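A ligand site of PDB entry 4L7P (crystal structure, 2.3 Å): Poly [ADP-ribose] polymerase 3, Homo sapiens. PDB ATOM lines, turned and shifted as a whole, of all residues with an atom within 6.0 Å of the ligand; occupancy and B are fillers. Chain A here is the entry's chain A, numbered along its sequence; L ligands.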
ATOM      1  N   ASP A 109      -5.799  -9.434  15.070  1.00  0.00           N
ATOM      2  CA  ASP A 109      -4.664 -10.187  14.509  1.00  0.00           C
ATOM      3  C   ASP A 109      -4.721 -11.643  14.941  1.00  0.00           C
ATOM      4  O   ASP A 109      -4.502 -12.541  14.134  1.00  0.00           O
ATOM      5  CB  ASP A 109      -3.329  -9.549  14.945  1.00  0.00           C
ATOM      6  CG  ASP A 109      -3.019  -8.203  14.305  1.00  0.00           C
ATOM      7  OD1 ASP A 109      -3.808  -7.768  13.425  1.00  0.00           O
ATOM      8  OD2 ASP A 109      -1.995  -7.593  14.674  1.00  0.00           O
ATOM      9  N   MET A 110      -5.088 -11.879  16.218  1.00  0.00           N
ATOM     10  CA  MET A 110      -5.285 -13.181  16.825  1.00  0.00           C
ATOM     11  C   MET A 110      -6.384 -13.952  16.048  1.00  0.00           C
ATOM     12  O   MET A 110      -6.185 -15.121  15.758  1.00  0.00           O
ATOM     13  CB  MET A 110      -5.631 -13.027  18.319  1.00  0.00           C
ATOM     14  CG  MET A 110      -5.987 -14.342  19.031  1.00  0.00           C
ATOM     15  SD  MET A 110      -7.730 -14.799  18.797  1.00  0.00           S
ATOM     16  CE  MET A 110      -8.525 -13.580  19.924  1.00  0.00           C
ATOM     17  N   LEU A 112      -7.388 -13.290  12.908  1.00  0.00           N
ATOM     18  CA  LEU A 112      -6.958 -13.482  11.509  1.00  0.00           C
ATOM     19  C   LEU A 112      -6.094 -14.738  11.429  1.00  0.00           C
ATOM     20  O   LEU A 112      -6.178 -15.475  10.460  1.00  0.00           O
ATOM     21  CB  LEU A 112      -6.212 -12.240  10.954  1.00  0.00           C
ATOM     22  CG  LEU A 112      -7.086 -10.953  10.744  1.00  0.00           C
ATOM     23  CD1 LEU A 112      -6.221  -9.732  10.480  1.00  0.00           C
ATOM     24  CD2 LEU A 112      -8.122 -11.117   9.649  1.00  0.00           C
ATOM     25  N   VAL A 113      -5.289 -14.991  12.465  1.00  0.00           N
ATOM     26  CA  VAL A 113      -4.450 -16.194  12.561  1.00  0.00           C
ATOM     27  C   VAL A 113      -5.400 -17.407  12.752  1.00  0.00           C
ATOM     28  O   VAL A 113      -5.346 -18.354  11.970  1.00  0.00           O
ATOM     29  CB  VAL A 113      -3.377 -16.078  13.697  1.00  0.00           C
ATOM     30  CG1 VAL A 113      -2.664 -17.418  13.940  1.00  0.00           C
ATOM     31  CG2 VAL A 113      -2.359 -14.984  13.384  1.00  0.00           C
ATOM     32  N   TRP A 208      10.297  -9.938   0.698  1.00  0.00           N
ATOM     33  CA  TRP A 208      10.054 -10.872   1.786  1.00  0.00           C
ATOM     34  C   TRP A 208       8.685 -10.674   2.423  1.00  0.00           C
ATOM     35  O   TRP A 208       8.201  -9.536   2.576  1.00  0.00           O
ATOM     36  CB  TRP A 208      11.106 -10.703   2.886  1.00  0.00           C
ATOM     37  CG  TRP A 208      12.518 -10.905   2.441  1.00  0.00           C
ATOM     38  CD1 TRP A 208      13.433  -9.943   2.147  1.00  0.00           C
ATOM     39  CD2 TRP A 208      13.187 -12.165   2.287  1.00  0.00           C
ATOM     40  NE1 TRP A 208      14.652 -10.532   1.859  1.00  0.00           N
ATOM     41  CE2 TRP A 208      14.511 -11.893   1.886  1.00  0.00           C
ATOM     42  CE3 TRP A 208      12.779 -13.506   2.417  1.00  0.00           C
ATOM     43  CZ2 TRP A 208      15.442 -12.908   1.636  1.00  0.00           C
ATOM     44  CZ3 TRP A 208      13.696 -14.508   2.143  1.00  0.00           C
ATOM     45  CH2 TRP A 208      15.006 -14.204   1.756  1.00  0.00           C
ATOM     46  N   HIS A 209       8.126 -11.812   2.905  1.00  0.00           N
ATOM     47  CA  HIS A 209       6.915 -11.849   3.691  1.00  0.00           C
ATOM     48  C   HIS A 209       7.072 -12.955   4.743  1.00  0.00           C
ATOM     49  O   HIS A 209       7.018 -14.146   4.417  1.00  0.00           O
ATOM     50  CB  HIS A 209       5.653 -11.996   2.853  1.00  0.00           C
ATOM     51  CG  HIS A 209       4.414 -11.905   3.675  1.00  0.00           C
ATOM     52  ND1 HIS A 209       3.871 -10.681   4.005  1.00  0.00           N
ATOM     53  CD2 HIS A 209       3.697 -12.881   4.268  1.00  0.00           C
ATOM     54  CE1 HIS A 209       2.833 -10.942   4.779  1.00  0.00           C
ATOM     55  NE2 HIS A 209       2.682 -12.260   4.968  1.00  0.00           N
ATOM     56  N   GLY A 210       7.357 -12.537   5.970  1.00  0.00           N
ATOM     57  CA  GLY A 210       7.539 -13.462   7.081  1.00  0.00           C
ATOM     58  C   GLY A 210       6.234 -13.683   7.811  1.00  0.00           C
ATOM     59  O   GLY A 210       5.446 -12.739   7.958  1.00  0.00           O
ATOM     60  N   THR A 211       6.023 -14.907   8.338  1.00  0.00           N
ATOM     61  CA  THR A 211       4.745 -15.167   9.004  1.00  0.00           C
ATOM     62  C   THR A 211       4.800 -16.307  10.050  1.00  0.00           C
ATOM     63  O   THR A 211       5.808 -16.992  10.195  1.00  0.00           O
ATOM     64  CB  THR A 211       3.718 -15.498   7.902  1.00  0.00           C
ATOM     65  OG1 THR A 211       2.407 -15.251   8.386  1.00  0.00           O
ATOM     66  CG2 THR A 211       3.862 -16.895   7.312  1.00  0.00           C
ATOM     67  N   ASN A 212       3.692 -16.446  10.818  1.00  0.00           N
ATOM     68  CA  ASN A 212       3.406 -17.523  11.762  1.00  0.00           C
ATOM     69  C   ASN A 212       3.449 -18.836  10.994  1.00  0.00           C
ATOM     70  O   ASN A 212       2.889 -18.878   9.901  1.00  0.00           O
ATOM     71  CB  ASN A 212       1.954 -17.324  12.309  1.00  0.00           C
ATOM     72  CG  ASN A 212       1.773 -16.553  13.583  1.00  0.00           C
ATOM     73  OD1 ASN A 212       2.083 -17.042  14.670  1.00  0.00           O
ATOM     74  ND2 ASN A 212       1.158 -15.382  13.483  1.00  0.00           N
ATOM     75  N   VAL A 215      -0.046 -20.104   9.656  1.00  0.00           N
ATOM     76  CA  VAL A 215      -0.794 -19.538   8.536  1.00  0.00           C
ATOM     77  C   VAL A 215      -0.137 -19.931   7.169  1.00  0.00           C
ATOM     78  O   VAL A 215      -0.680 -19.563   6.122  1.00  0.00           O
ATOM     79  CB  VAL A 215      -1.029 -17.998   8.688  1.00  0.00           C
ATOM     80  CG1 VAL A 215      -1.578 -17.633  10.074  1.00  0.00           C
ATOM     81  CG2 VAL A 215       0.200 -17.187   8.372  1.00  0.00           C
ATOM     82  N   TYR A 239       1.710  -6.439   3.294  1.00  0.00           N
ATOM     83  CA  TYR A 239       2.973  -5.924   3.759  1.00  0.00           C
ATOM     84  C   TYR A 239       4.127  -6.810   3.308  1.00  0.00           C
ATOM     85  O   TYR A 239       4.079  -8.024   3.463  1.00  0.00           O
ATOM     86  CB  TYR A 239       2.940  -5.834   5.294  1.00  0.00           C
ATOM     87  CG  TYR A 239       2.111  -4.700   5.833  1.00  0.00           C
ATOM     88  CD1 TYR A 239       2.702  -3.606   6.470  1.00  0.00           C
ATOM     89  CD2 TYR A 239       0.708  -4.723   5.768  1.00  0.00           C
ATOM     90  CE1 TYR A 239       1.950  -2.565   6.988  1.00  0.00           C
ATOM     91  CE2 TYR A 239      -0.058  -3.675   6.246  1.00  0.00           C
ATOM     92  CZ  TYR A 239       0.561  -2.595   6.871  1.00  0.00           C
ATOM     93  OH  TYR A 239      -0.174  -1.535   7.323  1.00  0.00           O
ATOM     94  N   PHE A 240       5.188  -6.170   2.808  1.00  0.00           N
ATOM     95  CA  PHE A 240       6.434  -6.781   2.346  1.00  0.00           C
ATOM     96  C   PHE A 240       7.642  -5.974   2.813  1.00  0.00           C
ATOM     97  O   PHE A 240       7.498  -4.792   3.114  1.00  0.00           O
ATOM     98  CB  PHE A 240       6.454  -6.866   0.809  1.00  0.00           C
ATOM     99  CG  PHE A 240       5.407  -7.748   0.174  1.00  0.00           C
ATOM    100  CD1 PHE A 240       5.662  -9.108  -0.035  1.00  0.00           C
ATOM    101  CD2 PHE A 240       4.208  -7.220  -0.264  1.00  0.00           C
ATOM    102  CE1 PHE A 240       4.706  -9.920  -0.664  1.00  0.00           C
ATOM    103  CE2 PHE A 240       3.263  -8.024  -0.895  1.00  0.00           C
ATOM    104  CZ  PHE A 240       3.515  -9.365  -1.092  1.00  0.00           C
ATOM    105  N   ALA A 241       8.830  -6.597   2.826  1.00  0.00           N
ATOM    106  CA  ALA A 241      10.085  -5.934   3.195  1.00  0.00           C
ATOM    107  C   ALA A 241      11.195  -6.282   2.182  1.00  0.00           C
ATOM    108  O   ALA A 241      11.208  -7.379   1.605  1.00  0.00           O
ATOM    109  CB  ALA A 241      10.514  -6.354   4.600  1.00  0.00           C
ATOM    110  N   LYS A 246      13.829  -7.481   8.763  1.00  0.00           N
ATOM    111  CA  LYS A 246      12.501  -6.880   9.048  1.00  0.00           C
ATOM    112  C   LYS A 246      11.388  -7.952   9.016  1.00  0.00           C
ATOM    113  O   LYS A 246      10.624  -8.041   9.973  1.00  0.00           O
ATOM    114  CB  LYS A 246      12.183  -5.722   8.075  1.00  0.00           C
ATOM    115  CG  LYS A 246      10.760  -5.177   8.167  1.00  0.00           C
ATOM    116  CD  LYS A 246      10.422  -4.533   9.522  1.00  0.00           C
ATOM    117  CE  LYS A 246       9.213  -3.649   9.419  1.00  0.00           C
ATOM    118  NZ  LYS A 246       8.494  -3.572  10.701  1.00  0.00           N
ATOM    119  N   SER A 247      11.316  -8.766   7.944  1.00  0.00           N
ATOM    120  CA  SER A 247      10.296  -9.834   7.854  1.00  0.00           C
ATOM    121  C   SER A 247      10.510 -10.982   8.887  1.00  0.00           C
ATOM    122  O   SER A 247       9.530 -11.564   9.342  1.00  0.00           O
ATOM    123  CB  SER A 247      10.277 -10.418   6.445  1.00  0.00           C
ATOM    124  OG  SER A 247       9.666  -9.519   5.540  1.00  0.00           O
ATOM    125  N   ALA A 248      11.771 -11.310   9.239  1.00  0.00           N
ATOM    126  CA  ALA A 248      12.134 -12.334  10.232  1.00  0.00           C
ATOM    127  C   ALA A 248      11.555 -12.014  11.613  1.00  0.00           C
ATOM    128  O   ALA A 248      11.376 -12.917  12.415  1.00  0.00           O
ATOM    129  CB  ALA A 248      13.645 -12.497  10.295  1.00  0.00           C
ATOM    130  N   GLY A 249      11.213 -10.731  11.861  1.00  0.00           N
ATOM    131  CA  GLY A 249      10.580 -10.286  13.097  1.00  0.00           C
ATOM    132  C   GLY A 249       9.165 -10.796  13.253  1.00  0.00           C
ATOM    133  O   GLY A 249       8.688 -10.987  14.377  1.00  0.00           O
ATOM    134  N   TYR A 250       8.464 -11.037  12.126  1.00  0.00           N
ATOM    135  CA  TYR A 250       7.092 -11.559  12.130  1.00  0.00           C
ATOM    136  C   TYR A 250       7.091 -13.072  11.946  1.00  0.00           C
ATOM    137  O   TYR A 250       6.020 -13.666  11.812  1.00  0.00           O
ATOM    138  CB  TYR A 250       6.234 -10.876  11.053  1.00  0.00           C
ATOM    139  CG  TYR A 250       6.277  -9.368  11.155  1.00  0.00           C
ATOM    140  CD1 TYR A 250       5.342  -8.677  11.934  1.00  0.00           C
ATOM    141  CD2 TYR A 250       7.243  -8.625  10.485  1.00  0.00           C
ATOM    142  CE1 TYR A 250       5.363  -7.286  12.013  1.00  0.00           C
ATOM    143  CE2 TYR A 250       7.297  -7.238  10.578  1.00  0.00           C
ATOM    144  CZ  TYR A 250       6.333  -6.575  11.334  1.00  0.00           C
ATOM    145  OH  TYR A 250       6.409  -5.219  11.462  1.00  0.00           O
ATOM    146  N   VAL A 251       8.276 -13.705  11.956  1.00  0.00           N
ATOM    147  CA  VAL A 251       8.374 -15.144  11.789  1.00  0.00           C
ATOM    148  C   VAL A 251       8.230 -15.785  13.146  1.00  0.00           C
ATOM    149  O   VAL A 251       9.103 -15.636  13.995  1.00  0.00           O
ATOM    150  CB  VAL A 251       9.665 -15.631  11.041  1.00  0.00           C
ATOM    151  CG1 VAL A 251       9.770 -17.160  11.055  1.00  0.00           C
ATOM    152  CG2 VAL A 251       9.690 -15.103   9.606  1.00  0.00           C
ATOM    153  N   ILE A 252       7.119 -16.482  13.358  1.00  0.00           N
ATOM    154  CA  ILE A 252       6.905 -17.225  14.599  1.00  0.00           C
ATOM    155  C   ILE A 252       7.198 -18.673  14.238  1.00  0.00           C
ATOM    156  O   ILE A 252       6.474 -19.310  13.455  1.00  0.00           O
ATOM    157  CB  ILE A 252       5.524 -16.976  15.285  1.00  0.00           C
ATOM    158  CG1 ILE A 252       5.358 -15.502  15.710  1.00  0.00           C
ATOM    159  CG2 ILE A 252       5.359 -17.877  16.524  1.00  0.00           C
ATOM    160  CD1 ILE A 252       4.603 -14.686  14.759  1.00  0.00           C
ATOM    161  N   SER A 338      12.082  -0.313   5.699  1.00  0.00           N
ATOM    162  CA  SER A 338      11.000  -0.089   4.757  1.00  0.00           C
ATOM    163  C   SER A 338       9.938  -1.172   4.804  1.00  0.00           C
ATOM    164  O   SER A 338      10.235  -2.346   5.023  1.00  0.00           O
ATOM    165  CB  SER A 338      11.529   0.002   3.322  1.00  0.00           C
ATOM    166  OG  SER A 338      12.350   1.146   3.122  1.00  0.00           O
ATOM    167  N   GLU A 339       8.700  -0.732   4.550  1.00  0.00           N
ATOM    168  CA  GLU A 339       7.519  -1.570   4.416  1.00  0.00           C
ATOM    169  C   GLU A 339       6.934  -1.230   3.054  1.00  0.00           C
ATOM    170  O   GLU A 339       6.650  -0.062   2.783  1.00  0.00           O
ATOM    171  CB  GLU A 339       6.528  -1.318   5.563  1.00  0.00           C
ATOM    172  CG  GLU A 339       7.151  -1.479   6.948  1.00  0.00           C
ATOM    173  CD  GLU A 339       6.184  -1.531   8.120  1.00  0.00           C
ATOM    174  OE1 GLU A 339       4.961  -1.620   7.878  1.00  0.00           O
ATOM    175  OE2 GLU A 339       6.648  -1.355   9.257  1.00  0.00           O
ATOM    176  N   TYR A 340       6.836  -2.240   2.177  1.00  0.00           N
ATOM    177  CA  TYR A 340       6.307  -2.169   0.813  1.00  0.00           C
ATOM    178  C   TYR A 340       4.839  -2.635   0.831  1.00  0.00           C
ATOM    179  O   TYR A 340       4.555  -3.732   1.344  1.00  0.00           O
ATOM    180  CB  TYR A 340       7.161  -3.053  -0.126  1.00  0.00           C
ATOM    181  CG  TYR A 340       8.533  -2.491  -0.423  1.00  0.00           C
ATOM    182  CD1 TYR A 340       8.887  -2.103  -1.713  1.00  0.00           C
ATOM    183  CD2 TYR A 340       9.535  -2.452   0.559  1.00  0.00           C
ATOM    184  CE1 TYR A 340      10.170  -1.652  -2.027  1.00  0.00           C
ATOM    185  CE2 TYR A 340      10.817  -1.973   0.260  1.00  0.00           C
ATOM    186  CZ  TYR A 340      11.126  -1.584  -1.027  1.00  0.00           C
ATOM    187  OH  TYR A 340      12.365  -1.097  -1.372  1.00  0.00           O
HETATM  188  C1  LIG L   1       1.851  -9.680  14.740  1.00  0.00           C
HETATM  189  C2  LIG L   1       3.216  -9.542  15.155  1.00  0.00           C
HETATM  190  C3  LIG L   1       4.155 -10.557  14.808  1.00  0.00           C
HETATM  191  C4  LIG L   1       3.748 -11.672  14.016  1.00  0.00           C
HETATM  192  C5  LIG L   1       2.378 -11.801  13.611  1.00  0.00           C
HETATM  193  C6  LIG L   1       1.403 -10.798  13.960  1.00  0.00           C
HETATM  194  C7  LIG L   1       0.022 -10.858  13.586  1.00  0.00           C
HETATM  195  C8  LIG L   1      -0.316 -11.156  12.106  1.00  0.00           C
HETATM  196  C9  LIG L   1      -1.710 -10.671  11.794  1.00  0.00           C
HETATM  197  O1  LIG L   1      -2.321 -11.501  10.780  1.00  0.00           O
HETATM  198  N1  LIG L   1       0.719 -10.414  11.287  1.00  0.00           N
HETATM  199  C10 LIG L   1       1.471 -10.973  10.330  1.00  0.00           C
HETATM  200  O2  LIG L   1       1.388 -12.137  10.013  1.00  0.00           O
HETATM  201  C11 LIG L   1       2.453  -9.996   9.701  1.00  0.00           C
HETATM  202  C12 LIG L   1       3.411 -10.402   8.608  1.00  0.00           C
HETATM  203  C13 LIG L   1       4.289  -9.421   8.111  1.00  0.00           C
HETATM  204  N2  LIG L   1       4.205  -8.020   8.340  1.00  0.00           N
HETATM  205  C14 LIG L   1       5.116  -7.215   7.816  1.00  0.00           C
HETATM  206  C15 LIG L   1       5.022  -5.828   8.030  1.00  0.00           C
HETATM  207  C16 LIG L   1       5.975  -4.982   7.477  1.00  0.00           C
HETATM  208  C17 LIG L   1       6.993  -5.521   6.703  1.00  0.00           C
HETATM  209  C18 LIG L   1       7.130  -6.864   6.513  1.00  0.00           C
HETATM  210  C19 LIG L   1       6.191  -7.748   7.036  1.00  0.00           C
HETATM  211  C20 LIG L   1       6.271  -9.178   6.860  1.00  0.00           C
HETATM  212  O3  LIG L   1       7.090  -9.765   6.224  1.00  0.00           O
HETATM  213  N3  LIG L   1       5.364  -9.954   7.423  1.00  0.00           N
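The side-chain hydroxyl of Ser 247 sits at hydrogen-bond distance from an oxygen (O3) of the ligand. The backbone NH (N) of Gly 210 lies within hydrogen-bond range of an oxygen (O3) of the ligand (2.8 Å).
Residues that only touch the ligand: Ile 252 (3.2 Å), His 209 (3.3 Å), Tyr 239 (3.4 Å), Glu 339 (3.5 Å), Tyr 250 (3.5 Å), Thr 211 (3.7 Å), Phe 240 (3.7 Å), Asp 109 (3.7 Å), Asn 212 (3.8 Å), Trp 208 (3.8 Å), Ala 241 (3.9 Å), Leu 112 (3.96 Å) and Lys 246 (3.98 Å). Hydrophobic or aromatic side chains within 4 Å of the ligand: Leu 112, His 209, Tyr 239, Ala 241, Tyr 250 and Ile 252. Of the 23 residues printed, 15 come within 4 Å of the ligand.
The backbone carbonyl oxygen of Trp 208 lies close to the side-chain hydroxyl of Ser 247 (3.3 Å). The backbone NH of Ile 252 lies within hydrogen-bond range of the backbone carbonyl oxygen of Thr 211 (3.5 Å). A ring nitrogen (ND1) of His 209 sits at hydrogen-bond distance from the backbone carbonyl oxygen (O) of Tyr 239 (2.7 Å). The side-chain carboxylate (OE2) of Glu 339 is in salt-bridge range of the side-chain amino group (NZ) of Lys 246, at 3.2 Å. NZ of Lys 246 is in hydrogen-bond range of OH of Tyr 250, at 2.8 Å. O of Phe 240 sits at hydrogen-bond distance from N of Tyr 340 (2.8 Å). The backbone NH (N) of Trp 208 lies within hydrogen-bond range of the backbone carbonyl oxygen (O) of Ala 241, 2.9 Å away.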
